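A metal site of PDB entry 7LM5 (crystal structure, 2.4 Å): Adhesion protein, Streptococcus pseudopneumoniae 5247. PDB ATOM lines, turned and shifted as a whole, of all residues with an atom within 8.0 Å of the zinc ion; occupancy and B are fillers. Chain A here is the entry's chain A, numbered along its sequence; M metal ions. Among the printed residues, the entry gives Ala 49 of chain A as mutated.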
ATOM      1  N   PHE A  22      -9.509  16.221  -8.847  1.00  0.00           N
ATOM      2  CA  PHE A  22      -8.514  17.254  -9.209  1.00  0.00           C
ATOM      3  C   PHE A  22      -9.227  18.589  -9.449  1.00  0.00           C
ATOM      4  O   PHE A  22     -10.436  18.615  -9.414  1.00  0.00           O
ATOM      5  CB  PHE A  22      -7.512  16.754 -10.261  1.00  0.00           C
ATOM      6  CG  PHE A  22      -7.907  16.881 -11.709  1.00  0.00           C
ATOM      7  CD1 PHE A  22      -9.120  16.406 -12.150  1.00  0.00           C
ATOM      8  CD2 PHE A  22      -7.047  17.436 -12.620  1.00  0.00           C
ATOM      9  CE1 PHE A  22      -9.486  16.522 -13.481  1.00  0.00           C
ATOM     10  CE2 PHE A  22      -7.412  17.543 -13.948  1.00  0.00           C
ATOM     11  CZ  PHE A  22      -8.628  17.095 -14.365  1.00  0.00           C
ATOM     12  N   ALA A  49      -1.173  13.907 -13.041  1.00  0.00           N
ATOM     13  CA  ALA A  49      -0.210  13.259 -13.924  1.00  0.00           C
ATOM     14  C   ALA A  49       0.151  11.867 -13.408  1.00  0.00           C
ATOM     15  O   ALA A  49      -0.194  10.859 -14.023  1.00  0.00           O
ATOM     16  CB  ALA A  49       1.028  14.119 -14.069  1.00  0.00           C
ATOM     17  N   PHE A  51      -0.928  10.747 -10.423  1.00  0.00           N
ATOM     18  CA  PHE A  51      -2.176  10.315  -9.795  1.00  0.00           C
ATOM     19  C   PHE A  51      -1.825   9.329  -8.677  1.00  0.00           C
ATOM     20  O   PHE A  51      -0.892   9.612  -7.903  1.00  0.00           O
ATOM     21  CB  PHE A  51      -3.130   9.783 -10.861  1.00  0.00           C
ATOM     22  CG  PHE A  51      -3.633  10.851 -11.799  1.00  0.00           C
ATOM     23  CD1 PHE A  51      -4.535  11.807 -11.368  1.00  0.00           C
ATOM     24  CD2 PHE A  51      -3.189  10.890 -13.108  1.00  0.00           C
ATOM     25  CE1 PHE A  51      -4.992  12.787 -12.222  1.00  0.00           C
ATOM     26  CE2 PHE A  51      -3.645  11.867 -13.971  1.00  0.00           C
ATOM     27  CZ  PHE A  51      -4.546  12.816 -13.528  1.00  0.00           C
ATOM     28  N   LEU A  74      -8.921   9.205 -17.475  1.00  0.00           N
ATOM     29  CA  LEU A  74      -7.944   9.987 -16.747  1.00  0.00           C
ATOM     30  C   LEU A  74      -7.638   9.332 -15.402  1.00  0.00           C
ATOM     31  O   LEU A  74      -6.598   8.700 -15.236  1.00  0.00           O
ATOM     32  CB  LEU A  74      -8.435  11.421 -16.538  1.00  0.00           C
ATOM     33  CG  LEU A  74      -7.443  12.383 -15.884  1.00  0.00           C
ATOM     34  CD1 LEU A  74      -6.183  12.525 -16.730  1.00  0.00           C
ATOM     35  CD2 LEU A  74      -8.087  13.739 -15.642  1.00  0.00           C
ATOM     36  N   ASP A 123      -8.881  11.183 -25.808  1.00  0.00           N
ATOM     37  CA  ASP A 123      -8.355  12.396 -25.141  1.00  0.00           C
ATOM     38  C   ASP A 123      -9.300  12.813 -24.026  1.00  0.00           C
ATOM     39  O   ASP A 123     -10.453  12.945 -24.293  1.00  0.00           O
ATOM     40  CB  ASP A 123      -8.196  13.488 -26.181  1.00  0.00           C
ATOM     41  CG  ASP A 123      -7.518  14.726 -25.679  1.00  0.00           C
ATOM     42  OD1 ASP A 123      -7.277  14.806 -24.515  1.00  0.00           O
ATOM     43  OD2 ASP A 123      -7.230  15.578 -26.480  1.00  0.00           O
ATOM     44  N   PRO A 124      -8.850  12.997 -22.765  1.00  0.00           N
ATOM     45  CA  PRO A 124      -9.723  13.400 -21.694  1.00  0.00           C
ATOM     46  C   PRO A 124      -9.809  14.900 -21.402  1.00  0.00           C
ATOM     47  O   PRO A 124     -10.701  15.271 -20.747  1.00  0.00           O
ATOM     48  CB  PRO A 124      -9.016  12.785 -20.496  1.00  0.00           C
ATOM     49  CG  PRO A 124      -7.601  12.976 -20.822  1.00  0.00           C
ATOM     50  CD  PRO A 124      -7.518  12.723 -22.302  1.00  0.00           C
ATOM     51  N   HIS A 125      -8.911  15.721 -21.963  1.00  0.00           N
ATOM     52  CA  HIS A 125      -8.801  17.177 -21.713  1.00  0.00           C
ATOM     53  C   HIS A 125      -9.962  18.004 -22.302  1.00  0.00           C
ATOM     54  O   HIS A 125      -9.701  18.912 -23.036  1.00  0.00           O
ATOM     55  CB  HIS A 125      -7.473  17.701 -22.247  1.00  0.00           C
ATOM     56  CG  HIS A 125      -6.239  17.064 -21.711  1.00  0.00           C
ATOM     57  ND1 HIS A 125      -5.571  16.085 -22.362  1.00  0.00           N
ATOM     58  CD2 HIS A 125      -5.491  17.321 -20.640  1.00  0.00           C
ATOM     59  CE1 HIS A 125      -4.526  15.724 -21.685  1.00  0.00           C
ATOM     60  NE2 HIS A 125      -4.436  16.465 -20.635  1.00  0.00           N
ATOM     61  N   TRP A 127     -12.206  19.666 -20.318  1.00  0.00           N
ATOM     62  CA  TRP A 127     -12.550  20.796 -19.463  1.00  0.00           C
ATOM     63  C   TRP A 127     -12.001  22.122 -19.987  1.00  0.00           C
ATOM     64  O   TRP A 127     -12.471  23.180 -19.552  1.00  0.00           O
ATOM     65  CB  TRP A 127     -12.063  20.547 -18.044  1.00  0.00           C
ATOM     66  CG  TRP A 127     -10.579  20.345 -17.932  1.00  0.00           C
ATOM     67  CD1 TRP A 127      -9.629  21.320 -17.797  1.00  0.00           C
ATOM     68  CD2 TRP A 127      -9.880  19.095 -17.929  1.00  0.00           C
ATOM     69  NE1 TRP A 127      -8.381  20.748 -17.719  1.00  0.00           N
ATOM     70  CE2 TRP A 127      -8.503  19.385 -17.796  1.00  0.00           C
ATOM     71  CE3 TRP A 127     -10.285  17.762 -18.036  1.00  0.00           C
ATOM     72  CZ2 TRP A 127      -7.536  18.391 -17.773  1.00  0.00           C
ATOM     73  CZ3 TRP A 127      -9.319  16.771 -18.002  1.00  0.00           C
ATOM     74  CH2 TRP A 127      -7.955  17.090 -17.867  1.00  0.00           C
ATOM     75  N   LEU A 128     -11.026  22.089 -20.895  1.00  0.00           N
ATOM     76  CA  LEU A 128     -10.487  23.324 -21.448  1.00  0.00           C
ATOM     77  C   LEU A 128     -11.331  23.889 -22.589  1.00  0.00           C
ATOM     78  O   LEU A 128     -11.055  24.999 -23.051  1.00  0.00           O
ATOM     79  CB  LEU A 128      -9.051  23.101 -21.910  1.00  0.00           C
ATOM     80  CG  LEU A 128      -8.096  22.744 -20.764  1.00  0.00           C
ATOM     81  CD1 LEU A 128      -6.686  22.494 -21.282  1.00  0.00           C
ATOM     82  CD2 LEU A 128      -8.099  23.839 -19.711  1.00  0.00           C
ATOM     83  N   HIS A 189       2.495  19.687 -23.158  1.00  0.00           N
ATOM     84  CA  HIS A 189       1.962  18.359 -23.446  1.00  0.00           C
ATOM     85  C   HIS A 189       0.606  18.506 -24.126  1.00  0.00           C
ATOM     86  O   HIS A 189       0.033  19.588 -24.186  1.00  0.00           O
ATOM     87  CB  HIS A 189       1.867  17.494 -22.180  1.00  0.00           C
ATOM     88  CG  HIS A 189       0.733  17.833 -21.271  1.00  0.00           C
ATOM     89  ND1 HIS A 189       0.711  18.972 -20.497  1.00  0.00           N
ATOM     90  CD2 HIS A 189      -0.416  17.168 -20.994  1.00  0.00           C
ATOM     91  CE1 HIS A 189      -0.401  19.003 -19.800  1.00  0.00           C
ATOM     92  NE2 HIS A 189      -1.108  17.922 -20.073  1.00  0.00           N
ATOM     93  N   THR A 190       0.119  17.389 -24.670  1.00  0.00           N
ATOM     94  CA  THR A 190      -1.080  17.392 -25.525  1.00  0.00           C
ATOM     95  C   THR A 190      -2.313  17.499 -24.645  1.00  0.00           C
ATOM     96  O   THR A 190      -2.981  16.511 -24.301  1.00  0.00           O
ATOM     97  CB  THR A 190      -1.107  16.142 -26.398  1.00  0.00           C
ATOM     98  OG1 THR A 190       0.157  15.982 -27.046  1.00  0.00           O
ATOM     99  CG2 THR A 190      -2.201  16.252 -27.449  1.00  0.00           C
ATOM    100  N   ALA A 191      -2.638  18.740 -24.269  1.00  0.00           N
ATOM    101  CA  ALA A 191      -3.755  19.004 -23.382  1.00  0.00           C
ATOM    102  C   ALA A 191      -4.772  19.998 -23.933  1.00  0.00           C
ATOM    103  O   ALA A 191      -5.851  20.137 -23.354  1.00  0.00           O
ATOM    104  CB  ALA A 191      -3.249  19.527 -22.025  1.00  0.00           C
ATOM    105  N   PHE A 192      -4.465  20.700 -25.016  1.00  0.00           N
ATOM    106  CA  PHE A 192      -5.318  21.767 -25.537  1.00  0.00           C
ATOM    107  C   PHE A 192      -5.960  21.395 -26.865  1.00  0.00           C
ATOM    108  O   PHE A 192      -6.247  22.273 -27.686  1.00  0.00           O
ATOM    109  CB  PHE A 192      -4.523  23.065 -25.673  1.00  0.00           C
ATOM    110  CG  PHE A 192      -3.941  23.552 -24.365  1.00  0.00           C
ATOM    111  CD1 PHE A 192      -4.651  24.411 -23.553  1.00  0.00           C
ATOM    112  CD2 PHE A 192      -2.675  23.142 -23.966  1.00  0.00           C
ATOM    113  CE1 PHE A 192      -4.123  24.854 -22.361  1.00  0.00           C
ATOM    114  CE2 PHE A 192      -2.138  23.586 -22.773  1.00  0.00           C
ATOM    115  CZ  PHE A 192      -2.867  24.442 -21.971  1.00  0.00           C
ATOM    116  N   GLY A 208       2.930  13.680 -24.797  1.00  0.00           N
ATOM    117  CA  GLY A 208       1.642  13.140 -25.184  1.00  0.00           C
ATOM    118  C   GLY A 208       0.516  13.609 -24.295  1.00  0.00           C
ATOM    119  O   GLY A 208       0.563  14.692 -23.690  1.00  0.00           O
ATOM    120  N   ILE A 209      -0.523  12.773 -24.210  1.00  0.00           N
ATOM    121  CA  ILE A 209      -1.674  13.087 -23.356  1.00  0.00           C
ATOM    122  C   ILE A 209      -1.230  13.294 -21.915  1.00  0.00           C
ATOM    123  O   ILE A 209      -1.701  14.206 -21.229  1.00  0.00           O
ATOM    124  CB  ILE A 209      -2.734  11.982 -23.474  1.00  0.00           C
ATOM    125  CG1 ILE A 209      -3.405  12.040 -24.845  1.00  0.00           C
ATOM    126  CG2 ILE A 209      -3.771  12.091 -22.360  1.00  0.00           C
ATOM    127  CD1 ILE A 209      -4.232  13.299 -25.061  1.00  0.00           C
ATOM    128  N   SER A 210      -0.317  12.449 -21.435  1.00  0.00           N
ATOM    129  CA  SER A 210       0.223  12.620 -20.094  1.00  0.00           C
ATOM    130  C   SER A 210       1.564  13.335 -20.148  1.00  0.00           C
ATOM    131  O   SER A 210       2.347  13.104 -21.079  1.00  0.00           O
ATOM    132  CB  SER A 210       0.407  11.264 -19.409  1.00  0.00           C
ATOM    133  OG  SER A 210      -0.824  10.561 -19.343  1.00  0.00           O
ATOM    134  N   PRO A 211       1.855  14.208 -19.183  1.00  0.00           N
ATOM    135  CA  PRO A 211       3.146  14.901 -19.183  1.00  0.00           C
ATOM    136  C   PRO A 211       4.335  13.977 -19.043  1.00  0.00           C
ATOM    137  O   PRO A 211       5.451  14.359 -19.407  1.00  0.00           O
ATOM    138  CB  PRO A 211       3.042  15.860 -17.977  1.00  0.00           C
ATOM    139  CG  PRO A 211       1.570  15.964 -17.694  1.00  0.00           C
ATOM    140  CD  PRO A 211       0.989  14.632 -18.067  1.00  0.00           C
ATOM    141  N   GLU A 238       4.466  24.950 -18.765  1.00  0.00           N
ATOM    142  CA  GLU A 238       3.599  24.838 -17.601  1.00  0.00           C
ATOM    143  C   GLU A 238       4.358  25.273 -16.356  1.00  0.00           C
ATOM    144  O   GLU A 238       5.570  25.068 -16.244  1.00  0.00           O
ATOM    145  CB  GLU A 238       3.077  23.407 -17.432  1.00  0.00           C
ATOM    146  CG  GLU A 238       2.010  23.005 -18.430  1.00  0.00           C
ATOM    147  CD  GLU A 238       1.685  21.530 -18.386  1.00  0.00           C
ATOM    148  OE1 GLU A 238       2.022  20.816 -19.353  1.00  0.00           O
ATOM    149  OE2 GLU A 238       1.105  21.076 -17.374  1.00  0.00           O
ATOM    150  N   PRO A 262      -2.879  24.321 -18.246  1.00  0.00           N
ATOM    151  CA  PRO A 262      -4.017  23.454 -18.589  1.00  0.00           C
ATOM    152  C   PRO A 262      -5.004  23.243 -17.448  1.00  0.00           C
ATOM    153  O   PRO A 262      -5.931  22.451 -17.604  1.00  0.00           O
ATOM    154  CB  PRO A 262      -3.332  22.129 -18.971  1.00  0.00           C
ATOM    155  CG  PRO A 262      -2.072  22.126 -18.175  1.00  0.00           C
ATOM    156  CD  PRO A 262      -1.625  23.559 -18.101  1.00  0.00           C
ATOM    157  N   GLU A 264      -4.693  21.687 -14.638  1.00  0.00           N
ATOM    158  CA  GLU A 264      -4.651  20.360 -14.038  1.00  0.00           C
ATOM    159  C   GLU A 264      -4.242  20.403 -12.579  1.00  0.00           C
ATOM    160  O   GLU A 264      -4.476  19.425 -11.848  1.00  0.00           O
ATOM    161  CB  GLU A 264      -3.696  19.448 -14.817  1.00  0.00           C
ATOM    162  CG  GLU A 264      -4.175  19.181 -16.235  1.00  0.00           C
ATOM    163  CD  GLU A 264      -3.276  18.217 -16.993  1.00  0.00           C
ATOM    164  OE1 GLU A 264      -2.288  17.727 -16.400  1.00  0.00           O
ATOM    165  OE2 GLU A 264      -3.559  17.953 -18.177  1.00  0.00           O
HETATM  166 ZN    ZN M   1      -3.009  16.500 -19.326  1.00  0.00          ZN
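ND1 of His 189 is in hydrogen-bond range of OE1 of Glu 238, at 2.5 Å.
ND1 of His 125 is in hydrogen-bond range of OD1 of Asp 123 (3.0 Å).
ND1 of His 125 lies close to O of Thr 190 (3.3 Å).
O of Ile 209 touches the zinc ion, 3.3 Å away.
Four residues have an atom within 4 Å of the zinc ion: His 125, His 189, Ile 209 and Glu 264.
The zinc ion is bound by the side-chain carboxylate (OE2) of Glu 264 (1.9 Å), a ring nitrogen (NE2) of His 125 (1.9 Å) and a ring nitrogen (NE2) of His 189 (2.5 Å).
The zinc ion has three donor atoms within binding distance.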
